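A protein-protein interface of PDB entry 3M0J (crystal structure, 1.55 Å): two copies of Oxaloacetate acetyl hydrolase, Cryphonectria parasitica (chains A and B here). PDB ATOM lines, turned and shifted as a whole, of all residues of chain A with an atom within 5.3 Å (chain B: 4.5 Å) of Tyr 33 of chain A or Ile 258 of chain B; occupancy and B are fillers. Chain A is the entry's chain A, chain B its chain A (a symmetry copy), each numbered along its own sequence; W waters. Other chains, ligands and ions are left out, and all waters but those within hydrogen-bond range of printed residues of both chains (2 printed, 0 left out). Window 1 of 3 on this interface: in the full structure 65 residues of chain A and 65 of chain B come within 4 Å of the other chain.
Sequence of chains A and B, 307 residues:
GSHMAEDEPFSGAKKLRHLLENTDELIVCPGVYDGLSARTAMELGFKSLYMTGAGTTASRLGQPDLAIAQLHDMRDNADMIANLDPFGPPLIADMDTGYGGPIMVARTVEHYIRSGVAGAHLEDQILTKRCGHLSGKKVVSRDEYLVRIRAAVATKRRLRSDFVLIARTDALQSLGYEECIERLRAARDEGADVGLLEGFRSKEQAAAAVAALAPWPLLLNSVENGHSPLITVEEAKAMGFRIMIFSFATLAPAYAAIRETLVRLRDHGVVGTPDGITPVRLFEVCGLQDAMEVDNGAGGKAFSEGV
OD2 of Asp 34 of chain B sits at hydrogen-bond distance from OG of Ser 59 of chain A, at 2.7 Å.
The backbone carbonyl oxygen of Gly 31 of chain A sits at hydrogen-bond distance from the side-chain hydroxyl of Thr 250 of chain A, 2.7 Å away.
OD1 of Asp 34 of chain A sits at hydrogen-bond distance from OG of Ser 37 of chain A (2.6 Å).
The backbone carbonyl oxygen (O) of Ala 257 of chain B is in hydrogen-bond range of the side-chain hydroxyl (OG1) of Thr 261 of chain B.
The backbone carbonyl oxygen of Leu 36 of chain A lies within hydrogen-bond range of the side-chain hydroxyl of Thr 40 of chain A.
The side-chain hydroxyl (OG) of Ser 37 of chain A lies within hydrogen-bond range of the backbone NH (N) of Tyr 33 of chain A (2.9 Å).
The guanidinium group of Arg 259 of chain B lies within hydrogen-bond range of the side-chain hydroxyl of Tyr 255 of chain B (3.2 Å).
Among the printed residues, pairs that only touch across the chains: Tyr 33 of chain A with Asp 34 of chain B (3.8 Å), Tyr 33 of chain A with Ile 258 of chain B (3.9 Å), Asp 34 of chain A with Tyr 33 of chain B (3.8 Å), Leu 36 of chain A with Tyr 255 of chain B (3.9 Å), Thr 40 of chain A with Tyr 255 of chain B (3.3 Å), Thr 40 of chain A with Ile 258 of chain B (3.9 Å), Thr 40 of chain A with Arg 259 of chain B (3.6 Å), Leu 44 of chain A with Arg 259 of chain B (3.7 Å), Leu 44 of chain A with Leu 262 of chain B (3.4 Å), Thr 250 of chain A with Ile 258 of chain B (3.7 Å), Thr 250 of chain A with Leu 262 of chain B (3.8 Å), Pro 253 of chain A with Ala 257 of chain B (3.4 Å) and Pro 253 of chain A with Thr 261 of chain B (3.1 Å).
Of the printed residues of chain B, Tyr 33 of chain A touches Asp 34 and Ile 258.
Ile 258 of chain B touches three residues of chain A.
Of the printed residues of chain B, Thr 250 of chain A touches Ile 258 (3.7 Å) and Leu 262 (3.8 Å).
Of the printed residues of chain B, Ser 59 of chain A touches Asp 34.
Gly 35 of chain A touches none of the printed residues of chain B.
The nearest printed residue of chain B that does not touch Tyr 33 of chain A is Tyr 33 of chain B (4.005 Å).
Of the 23 printed residues of chain A, 8 touch a printed residue of chain B.
Hydrophobic or aromatic side chains of chain A that line the printed part of chain B: Tyr 33, Leu 36, Leu 44 and Pro 253.
Along chain A the printed residues that touch a printed residue of chain B span positions 33 to 253.
Printed residues of chain B that touch a printed residue of chain A: Tyr 33, Asp 34, Tyr 255, Ala 257, Ile 258, Arg 259, Thr 261 and Leu 262.
Hydrophobic or aromatic side chains of chain B within 4 Å of the printed part of chain A: Tyr 33, Tyr 255, Ala 257, Ile 258 and Leu 262.
Among the printed residues, 14 pairs touch across the chains.
Tyr 33 of chain A touches Asp 34 of chain B, and with the chains exchanged Asp 34 of chain A touches Tyr 33 of chain B.
Water W1 lies within hydrogen-bond range of OH of Tyr 33 of chain A (2.7 Å), OD2 of Asp 34 of chain B (2.8 Å) and OH of Tyr 33 of chain B (2.8 Å).
Water W2 lies within hydrogen-bond range of the side-chain hydroxyl of Tyr 33 of chain B (2.7 Å), the side-chain carboxylate of Asp 34 of chain A (2.8 Å) and the side-chain hydroxyl of Tyr 33 of chain A (2.8 Å).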
ATOM      1  N   GLY A  31     -29.827 -12.616 -13.819  1.00  0.00           N
ATOM      2  CA  GLY A  31     -28.730 -12.158 -14.637  1.00  0.00           C
ATOM      3  C   GLY A  31     -27.397 -12.567 -14.043  1.00  0.00           C
ATOM      4  O   GLY A  31     -27.060 -12.164 -12.928  1.00  0.00           O
ATOM      5  N   VAL A  32     -26.644 -13.353 -14.799  1.00  0.00           N
ATOM      6  CA  VAL A  32     -25.335 -13.841 -14.346  1.00  0.00           C
ATOM      7  C   VAL A  32     -24.281 -13.267 -15.253  1.00  0.00           C
ATOM      8  O   VAL A  32     -24.584 -12.801 -16.365  1.00  0.00           O
ATOM      9  CB  VAL A  32     -25.321 -15.370 -14.257  1.00  0.00           C
ATOM     10  CG1 VAL A  32     -26.410 -15.801 -13.319  1.00  0.00           C
ATOM     11  CG2 VAL A  32     -25.559 -15.997 -15.645  1.00  0.00           C
ATOM     12  N   TYR A  33     -23.032 -13.295 -14.803  1.00  0.00           N
ATOM     13  CA  TYR A  33     -21.981 -12.619 -15.560  1.00  0.00           C
ATOM     14  C   TYR A  33     -20.643 -13.337 -15.576  1.00  0.00           C
ATOM     15  O   TYR A  33     -19.701 -12.884 -16.211  1.00  0.00           O
ATOM     16  CB  TYR A  33     -21.799 -11.234 -14.942  1.00  0.00           C
ATOM     17  CG  TYR A  33     -21.282 -11.242 -13.516  1.00  0.00           C
ATOM     18  CD1 TYR A  33     -19.917 -11.261 -13.245  1.00  0.00           C
ATOM     19  CD2 TYR A  33     -22.165 -11.214 -12.436  1.00  0.00           C
ATOM     20  CE1 TYR A  33     -19.446 -11.241 -11.927  1.00  0.00           C
ATOM     21  CE2 TYR A  33     -21.716 -11.218 -11.143  1.00  0.00           C
ATOM     22  CZ  TYR A  33     -20.353 -11.222 -10.892  1.00  0.00           C
ATOM     23  OH  TYR A  33     -19.906 -11.210  -9.592  1.00  0.00           O
ATOM     24  N   ASP A  34     -20.560 -14.447 -14.860  1.00  0.00           N
ATOM     25  CA  ASP A  34     -19.321 -15.198 -14.783  1.00  0.00           C
ATOM     26  C   ASP A  34     -19.650 -16.616 -14.340  1.00  0.00           C
ATOM     27  O   ASP A  34     -20.822 -16.978 -14.232  1.00  0.00           O
ATOM     28  CB  ASP A  34     -18.297 -14.515 -13.855  1.00  0.00           C
ATOM     29  CG  ASP A  34     -18.588 -14.724 -12.372  1.00  0.00           C
ATOM     30  OD1 ASP A  34     -19.753 -14.972 -11.987  1.00  0.00           O
ATOM     31  OD2 ASP A  34     -17.636 -14.623 -11.557  1.00  0.00           O
ATOM     32  N   GLY A  35     -18.618 -17.416 -14.104  1.00  0.00           N
ATOM     33  CA  GLY A  35     -18.802 -18.809 -13.734  1.00  0.00           C
ATOM     34  C   GLY A  35     -19.421 -18.969 -12.355  1.00  0.00           C
ATOM     35  O   GLY A  35     -20.260 -19.838 -12.147  1.00  0.00           O
ATOM     36  N   LEU A  36     -19.021 -18.119 -11.417  1.00  0.00           N
ATOM     37  CA  LEU A  36     -19.506 -18.232 -10.039  1.00  0.00           C
ATOM     38  C   LEU A  36     -20.971 -17.843  -9.942  1.00  0.00           C
ATOM     39  O   LEU A  36     -21.777 -18.538  -9.309  1.00  0.00           O
ATOM     40  CB  LEU A  36     -18.661 -17.361  -9.102  1.00  0.00           C
ATOM     41  CG  LEU A  36     -19.041 -17.417  -7.614  1.00  0.00           C
ATOM     42  CD1 LEU A  36     -18.787 -18.823  -7.088  1.00  0.00           C
ATOM     43  CD2 LEU A  36     -18.273 -16.397  -6.795  1.00  0.00           C
ATOM     44  N   SER A  37     -21.325 -16.714 -10.547  1.00  0.00           N
ATOM     45  CA  SER A  37     -22.719 -16.296 -10.520  1.00  0.00           C
ATOM     46  C   SER A  37     -23.602 -17.339 -11.224  1.00  0.00           C
ATOM     47  O   SER A  37     -24.654 -17.710 -10.713  1.00  0.00           O
ATOM     48  CB  SER A  37     -22.889 -14.887 -11.111  1.00  0.00           C
ATOM     49  OG  SER A  37     -22.327 -14.801 -12.410  1.00  0.00           O
ATOM     50  N   ALA A  38     -23.163 -17.834 -12.382  1.00  0.00           N
ATOM     51  CA  ALA A  38     -23.948 -18.826 -13.105  1.00  0.00           C
ATOM     52  C   ALA A  38     -24.077 -20.127 -12.307  1.00  0.00           C
ATOM     53  O   ALA A  38     -25.158 -20.709 -12.235  1.00  0.00           O
ATOM     54  CB  ALA A  38     -23.356 -19.094 -14.495  1.00  0.00           C
ATOM     55  N   THR A  40     -24.023 -20.509  -9.153  1.00  0.00           N
ATOM     56  CA  THR A  40     -24.899 -20.262  -8.011  1.00  0.00           C
ATOM     57  C   THR A  40     -26.367 -20.295  -8.427  1.00  0.00           C
ATOM     58  O   THR A  40     -27.177 -20.946  -7.781  1.00  0.00           O
ATOM     59  CB  THR A  40     -24.541 -18.944  -7.301  1.00  0.00           C
ATOM     60  OG1 THR A  40     -23.143 -18.956  -7.001  1.00  0.00           O
ATOM     61  CG2 THR A  40     -25.334 -18.773  -6.000  1.00  0.00           C
ATOM     62  N   LEU A  44     -29.267 -23.195  -7.297  1.00  0.00           N
ATOM     63  CA  LEU A  44     -30.546 -22.860  -6.682  1.00  0.00           C
ATOM     64  C   LEU A  44     -31.739 -23.306  -7.513  1.00  0.00           C
ATOM     65  O   LEU A  44     -32.880 -23.098  -7.115  1.00  0.00           O
ATOM     66  CB  LEU A  44     -30.641 -21.352  -6.401  1.00  0.00           C
ATOM     67  CG  LEU A  44     -29.614 -20.872  -5.369  1.00  0.00           C
ATOM     68  CD1 LEU A  44     -29.592 -19.356  -5.269  1.00  0.00           C
ATOM     69  CD2 LEU A  44     -29.901 -21.509  -4.003  1.00  0.00           C
ATOM     70  N   TYR A  50     -29.829 -15.675 -17.529  1.00  0.00           N
ATOM     71  CA  TYR A  50     -29.602 -14.581 -18.447  1.00  0.00           C
ATOM     72  C   TYR A  50     -28.163 -14.093 -18.295  1.00  0.00           C
ATOM     73  O   TYR A  50     -27.706 -13.862 -17.174  1.00  0.00           O
ATOM     74  CB  TYR A  50     -30.571 -13.439 -18.151  1.00  0.00           C
ATOM     75  CG  TYR A  50     -30.172 -12.174 -18.835  1.00  0.00           C
ATOM     76  CD1 TYR A  50     -30.178 -12.088 -20.229  1.00  0.00           C
ATOM     77  CD2 TYR A  50     -29.761 -11.069 -18.103  1.00  0.00           C
ATOM     78  CE1 TYR A  50     -29.795 -10.918 -20.877  1.00  0.00           C
ATOM     79  CE2 TYR A  50     -29.378  -9.906 -18.741  1.00  0.00           C
ATOM     80  CZ  TYR A  50     -29.398  -9.837 -20.118  1.00  0.00           C
ATOM     81  OH  TYR A  50     -29.014  -8.682 -20.729  1.00  0.00           O
ATOM     82  N   MET A  51     -27.455 -13.945 -19.418  1.00  0.00           N
ATOM     83  CA  MET A  51     -26.124 -13.351 -19.376  1.00  0.00           C
ATOM     84  C   MET A  51     -26.179 -11.877 -19.717  1.00  0.00           C
ATOM     85  O   MET A  51     -26.483 -11.500 -20.853  1.00  0.00           O
ATOM     86  CB  MET A  51     -25.154 -14.043 -20.332  1.00  0.00           C
ATOM     87  CG  MET A  51     -23.699 -13.598 -20.081  1.00  0.00           C
ATOM     88  SD  MET A  51     -22.564 -14.179 -21.342  1.00  0.00           S
ATOM     89  CE  MET A  51     -22.769 -12.882 -22.577  1.00  0.00           C
ATOM     90  N   THR A  52     -25.886 -11.054 -18.719  1.00  0.00           N
ATOM     91  CA  THR A  52     -25.860  -9.620 -18.870  1.00  0.00           C
ATOM     92  C   THR A  52     -24.617  -9.147 -19.613  1.00  0.00           C
ATOM     93  O   THR A  52     -23.497  -9.577 -19.308  1.00  0.00           O
ATOM     94  CB  THR A  52     -25.912  -8.928 -17.483  1.00  0.00           C
ATOM     95  OG1 THR A  52     -25.470  -7.577 -17.618  1.00  0.00           O
ATOM     96  CG2 THR A  52     -24.999  -9.618 -16.471  1.00  0.00           C
ATOM     97  N   GLY A  55     -22.761  -6.862 -17.141  1.00  0.00           N
ATOM     98  CA  GLY A  55     -22.033  -7.641 -16.149  1.00  0.00           C
ATOM     99  C   GLY A  55     -20.836  -8.329 -16.775  1.00  0.00           C
ATOM    100  O   GLY A  55     -19.753  -8.404 -16.198  1.00  0.00           O
ATOM    101  N   THR A  56     -21.024  -8.814 -17.993  1.00  0.00           N
ATOM    102  CA  THR A  56     -19.914  -9.436 -18.687  1.00  0.00           C
ATOM    103  C   THR A  56     -18.778  -8.425 -18.864  1.00  0.00           C
ATOM    104  O   THR A  56     -17.614  -8.745 -18.650  1.00  0.00           O
ATOM    105  CB  THR A  56     -20.346 -10.016 -20.055  1.00  0.00           C
ATOM    106  OG1 THR A  56     -21.277 -11.084 -19.850  1.00  0.00           O
ATOM    107  CG2 THR A  56     -19.131 -10.548 -20.818  1.00  0.00           C
ATOM    108  N   SER A  59     -17.039  -7.649 -15.467  1.00  0.00           N
ATOM    109  CA  SER A  59     -16.296  -8.763 -14.878  1.00  0.00           C
ATOM    110  C   SER A  59     -15.137  -9.241 -15.767  1.00  0.00           C
ATOM    111  O   SER A  59     -14.008  -9.398 -15.297  1.00  0.00           O
ATOM    112  CB  SER A  59     -17.255  -9.931 -14.590  1.00  0.00           C
ATOM    113  OG  SER A  59     -16.579 -11.046 -14.032  1.00  0.00           O
ATOM    114  N   ARG A  60     -15.421  -9.486 -17.049  1.00  0.00           N
ATOM    115  CA  ARG A  60     -14.384  -9.947 -17.963  1.00  0.00           C
ATOM    116  C   ARG A  60     -13.392  -8.856 -18.361  1.00  0.00           C
ATOM    117  O   ARG A  60     -12.237  -9.151 -18.673  1.00  0.00           O
ATOM    118  CB  ARG A  60     -14.993 -10.578 -19.214  1.00  0.00           C
ATOM    119  CG  ARG A  60     -15.398 -12.030 -19.044  1.00  0.00           C
ATOM    120  CD  ARG A  60     -15.850 -12.637 -20.376  1.00  0.00           C
ATOM    121  NE  ARG A  60     -14.752 -12.879 -21.315  1.00  0.00           N
ATOM    122  CZ  ARG A  60     -14.066 -14.020 -21.372  1.00  0.00           C
ATOM    123  NH1 ARG A  60     -14.359 -15.007 -20.539  1.00  0.00           N
ATOM    124  NH2 ARG A  60     -13.090 -14.172 -22.259  1.00  0.00           N
ATOM    125  N   ASN A  77     -17.937 -15.610 -23.072  1.00  0.00           N
ATOM    126  CA  ASN A  77     -18.603 -15.705 -21.781  1.00  0.00           C
ATOM    127  C   ASN A  77     -19.856 -16.563 -21.880  1.00  0.00           C
ATOM    128  O   ASN A  77     -20.128 -17.381 -21.004  1.00  0.00           O
ATOM    129  CB  ASN A  77     -18.964 -14.332 -21.239  1.00  0.00           C
ATOM    130  CG  ASN A  77     -18.930 -14.283 -19.719  1.00  0.00           C
ATOM    131  OD1 ASN A  77     -18.125 -14.964 -19.094  1.00  0.00           O
ATOM    132  ND2 ASN A  77     -19.789 -13.455 -19.121  1.00  0.00           N
ATOM    133  N   ILE A  81     -20.743 -20.080 -19.910  1.00  0.00           N
ATOM    134  CA  ILE A  81     -21.897 -20.184 -19.019  1.00  0.00           C
ATOM    135  C   ILE A  81     -22.919 -21.224 -19.489  1.00  0.00           C
ATOM    136  O   ILE A  81     -23.390 -22.054 -18.703  1.00  0.00           O
ATOM    137  CB  ILE A  81     -22.576 -18.808 -18.813  1.00  0.00           C
ATOM    138  CG1 ILE A  81     -21.645 -17.898 -18.010  1.00  0.00           C
ATOM    139  CG2 ILE A  81     -23.916 -18.965 -18.084  1.00  0.00           C
ATOM    140  CD1 ILE A  81     -22.072 -16.419 -18.000  1.00  0.00           C
ATOM    141  N   THR A 250     -26.928 -10.361  -9.779  1.00  0.00           N
ATOM    142  CA  THR A 250     -25.729 -10.922  -9.166  1.00  0.00           C
ATOM    143  C   THR A 250     -24.557  -9.922  -9.132  1.00  0.00           C
ATOM    144  O   THR A 250     -23.788  -9.889  -8.171  1.00  0.00           O
ATOM    145  CB  THR A 250     -25.309 -12.283  -9.808  1.00  0.00           C
ATOM    146  OG1 THR A 250     -24.953 -12.101 -11.183  1.00  0.00           O
ATOM    147  CG2 THR A 250     -26.457 -13.291  -9.741  1.00  0.00           C
ATOM    148  N   LEU A 251     -24.436  -9.083 -10.155  1.00  0.00           N
ATOM    149  CA  LEU A 251     -23.329  -8.127 -10.191  1.00  0.00           C
ATOM    150  C   LEU A 251     -23.424  -7.155  -9.020  1.00  0.00           C
ATOM    151  O   LEU A 251     -22.440  -6.867  -8.360  1.00  0.00           O
ATOM    152  CB  LEU A 251     -23.311  -7.340 -11.509  1.00  0.00           C
ATOM    153  CG  LEU A 251     -21.996  -6.594 -11.810  1.00  0.00           C
ATOM    154  CD1 LEU A 251     -20.882  -7.554 -12.277  1.00  0.00           C
ATOM    155  CD2 LEU A 251     -22.252  -5.543 -12.873  1.00  0.00           C
ATOM    156  N   PRO A 253     -25.141  -7.309  -5.902  1.00  0.00           N
ATOM    157  CA  PRO A 253     -24.794  -7.759  -4.549  1.00  0.00           C
ATOM    158  C   PRO A 253     -23.350  -8.222  -4.450  1.00  0.00           C
ATOM    159  O   PRO A 253     -22.774  -8.123  -3.370  1.00  0.00           O
ATOM    160  CB  PRO A 253     -25.753  -8.930  -4.307  1.00  0.00           C
ATOM    161  CG  PRO A 253     -26.119  -9.393  -5.704  1.00  0.00           C
ATOM    162  CD  PRO A 253     -26.230  -8.119  -6.479  1.00  0.00           C
ATOM    163  N   ALA A 254     -22.771  -8.725  -5.535  1.00  0.00           N
ATOM    164  CA  ALA A 254     -21.369  -9.118  -5.469  1.00  0.00           C
ATOM    165  C   ALA A 254     -20.523  -7.891  -5.142  1.00  0.00           C
ATOM    166  O   ALA A 254     -19.644  -7.941  -4.284  1.00  0.00           O
ATOM    167  CB  ALA A 254     -20.911  -9.765  -6.789  1.00  0.00           C
ATOM    168  N   TYR B  33     -10.255 -11.558  -8.702  1.00  0.00           N
ATOM    169  CA  TYR B  33     -10.420 -12.621  -9.690  1.00  0.00           C
ATOM    170  C   TYR B  33     -11.094 -12.195 -10.982  1.00  0.00           C
ATOM    171  O   TYR B  33     -11.250 -12.992 -11.896  1.00  0.00           O
ATOM    172  CB  TYR B  33     -11.250 -13.723  -9.033  1.00  0.00           C
ATOM    173  CG  TYR B  33     -12.670 -13.321  -8.681  1.00  0.00           C
ATOM    174  CD1 TYR B  33     -13.704 -13.446  -9.605  1.00  0.00           C
ATOM    175  CD2 TYR B  33     -12.978 -12.826  -7.414  1.00  0.00           C
ATOM    176  CE1 TYR B  33     -15.015 -13.098  -9.265  1.00  0.00           C
ATOM    177  CE2 TYR B  33     -14.254 -12.460  -7.079  1.00  0.00           C
ATOM    178  CZ  TYR B  33     -15.274 -12.607  -8.005  1.00  0.00           C
ATOM    179  OH  TYR B  33     -16.557 -12.253  -7.660  1.00  0.00           O
ATOM    180  N   ASP B  34     -11.509 -10.939 -11.044  1.00  0.00           N
ATOM    181  CA  ASP B  34     -12.189 -10.433 -12.221  1.00  0.00           C
ATOM    182  C   ASP B  34     -12.090  -8.914 -12.213  1.00  0.00           C
ATOM    183  O   ASP B  34     -11.401  -8.341 -11.369  1.00  0.00           O
ATOM    184  CB  ASP B  34     -13.649 -10.926 -12.293  1.00  0.00           C
ATOM    185  CG  ASP B  34     -14.588 -10.178 -11.352  1.00  0.00           C
ATOM    186  OD1 ASP B  34     -14.139  -9.616 -10.327  1.00  0.00           O
ATOM    187  OD2 ASP B  34     -15.815 -10.158 -11.625  1.00  0.00           O
ATOM    188  N   ALA B 254     -18.401 -12.675  -2.439  1.00  0.00           N
ATOM    189  CA  ALA B 254     -19.234 -12.531  -3.626  1.00  0.00           C
ATOM    190  C   ALA B 254     -20.213 -13.700  -3.693  1.00  0.00           C
ATOM    191  O   ALA B 254     -21.403 -13.514  -3.938  1.00  0.00           O
ATOM    192  CB  ALA B 254     -18.375 -12.462  -4.902  1.00  0.00           C
ATOM    193  N   TYR B 255     -19.718 -14.912  -3.464  1.00  0.00           N
ATOM    194  CA  TYR B 255     -20.600 -16.072  -3.501  1.00  0.00           C
ATOM    195  C   TYR B 255     -21.705 -15.960  -2.449  1.00  0.00           C
ATOM    196  O   TYR B 255     -22.888 -16.178  -2.749  1.00  0.00           O
ATOM    197  CB  TYR B 255     -19.827 -17.382  -3.305  1.00  0.00           C
ATOM    198  CG  TYR B 255     -20.768 -18.561  -3.122  1.00  0.00           C
ATOM    199  CD1 TYR B 255     -21.463 -19.090  -4.199  1.00  0.00           C
ATOM    200  CD2 TYR B 255     -20.986 -19.112  -1.866  1.00  0.00           C
ATOM    201  CE1 TYR B 255     -22.354 -20.144  -4.028  1.00  0.00           C
ATOM    202  CE2 TYR B 255     -21.859 -20.172  -1.687  1.00  0.00           C
ATOM    203  CZ  TYR B 255     -22.532 -20.689  -2.767  1.00  0.00           C
ATOM    204  OH  TYR B 255     -23.394 -21.744  -2.590  1.00  0.00           O
ATOM    205  N   ALA B 256     -21.328 -15.612  -1.220  1.00  0.00           N
ATOM    206  CA  ALA B 256     -22.307 -15.522  -0.136  1.00  0.00           C
ATOM    207  C   ALA B 256     -23.455 -14.570  -0.497  1.00  0.00           C
ATOM    208  O   ALA B 256     -24.633 -14.888  -0.301  1.00  0.00           O
ATOM    209  CB  ALA B 256     -21.626 -15.064   1.159  1.00  0.00           C
ATOM    210  N   ALA B 257     -23.089 -13.408  -1.030  1.00  0.00           N
ATOM    211  CA  ALA B 257     -24.041 -12.359  -1.406  1.00  0.00           C
ATOM    212  C   ALA B 257     -24.890 -12.741  -2.611  1.00  0.00           C
ATOM    213  O   ALA B 257     -26.109 -12.543  -2.611  1.00  0.00           O
ATOM    214  CB  ALA B 257     -23.305 -11.055  -1.667  1.00  0.00           C
ATOM    215  N   ILE B 258     -24.252 -13.279  -3.646  1.00  0.00           N
ATOM    216  CA  ILE B 258     -24.984 -13.747  -4.817  1.00  0.00           C
ATOM    217  C   ILE B 258     -25.999 -14.815  -4.422  1.00  0.00           C
ATOM    218  O   ILE B 258     -27.157 -14.757  -4.825  1.00  0.00           O
ATOM    219  CB  ILE B 258     -24.015 -14.312  -5.899  1.00  0.00           C
ATOM    220  CG1 ILE B 258     -23.202 -13.165  -6.512  1.00  0.00           C
ATOM    221  CG2 ILE B 258     -24.799 -15.068  -6.993  1.00  0.00           C
ATOM    222  CD1 ILE B 258     -21.943 -13.636  -7.250  1.00  0.00           C
ATOM    223  N   ARG B 259     -25.574 -15.773  -3.598  1.00  0.00           N
ATOM    224  CA  ARG B 259     -26.473 -16.846  -3.201  1.00  0.00           C
ATOM    225  C   ARG B 259     -27.658 -16.314  -2.386  1.00  0.00           C
ATOM    226  O   ARG B 259     -28.804 -16.678  -2.613  1.00  0.00           O
ATOM    227  CB  ARG B 259     -25.720 -17.912  -2.402  1.00  0.00           C
ATOM    228  CG  ARG B 259     -26.571 -19.143  -2.114  1.00  0.00           C
ATOM    229  CD  ARG B 259     -25.866 -20.130  -1.205  1.00  0.00           C
ATOM    230  NE  ARG B 259     -26.379 -21.474  -1.444  1.00  0.00           N
ATOM    231  CZ  ARG B 259     -27.577 -21.886  -1.051  1.00  0.00           C
ATOM    232  NH1 ARG B 259     -28.381 -21.061  -0.397  1.00  0.00           N
ATOM    233  NH2 ARG B 259     -27.974 -23.117  -1.320  1.00  0.00           N
ATOM    234  N   GLU B 260     -27.385 -15.443  -1.423  1.00  0.00           N
ATOM    235  CA  GLU B 260     -28.482 -14.952  -0.597  1.00  0.00           C
ATOM    236  C   GLU B 260     -29.460 -14.083  -1.406  1.00  0.00           C
ATOM    237  O   GLU B 260     -30.684 -14.166  -1.224  1.00  0.00           O
ATOM    238  CB  GLU B 260     -27.947 -14.275   0.658  1.00  0.00           C
ATOM    239  CG  GLU B 260     -27.930 -12.790   0.683  1.00  0.00           C
ATOM    240  CD  GLU B 260     -27.751 -12.292   2.107  1.00  0.00           C
ATOM    241  OE1 GLU B 260     -28.601 -11.511   2.582  1.00  0.00           O
ATOM    242  OE2 GLU B 260     -26.773 -12.716   2.758  1.00  0.00           O
ATOM    243  N   THR B 261     -28.928 -13.290  -2.331  1.00  0.00           N
ATOM    244  CA  THR B 261     -29.779 -12.511  -3.227  1.00  0.00           C
ATOM    245  C   THR B 261     -30.645 -13.396  -4.119  1.00  0.00           C
ATOM    246  O   THR B 261     -31.842 -13.154  -4.284  1.00  0.00           O
ATOM    247  CB  THR B 261     -28.930 -11.596  -4.136  1.00  0.00           C
ATOM    248  OG1 THR B 261     -28.174 -10.686  -3.326  1.00  0.00           O
ATOM    249  CG2 THR B 261     -29.825 -10.805  -5.075  1.00  0.00           C
ATOM    250  N   LEU B 262     -30.039 -14.415  -4.717  1.00  0.00           N
ATOM    251  CA  LEU B 262     -30.793 -15.276  -5.627  1.00  0.00           C
ATOM    252  C   LEU B 262     -31.835 -16.118  -4.886  1.00  0.00           C
ATOM    253  O   LEU B 262     -32.882 -16.449  -5.441  1.00  0.00           O
ATOM    254  CB  LEU B 262     -29.860 -16.156  -6.469  1.00  0.00           C
ATOM    255  CG  LEU B 262     -29.006 -15.405  -7.497  1.00  0.00           C
ATOM    256  CD1 LEU B 262     -28.214 -16.400  -8.334  1.00  0.00           C
ATOM    257  CD2 LEU B 262     -29.867 -14.504  -8.395  1.00  0.00           C
HETATM  258  O   HOH W   1     -17.439 -10.145  -9.351  1.00  0.00           O
HETATM  259  O   HOH W   2     -18.422 -13.581  -9.086  1.00  0.00           O
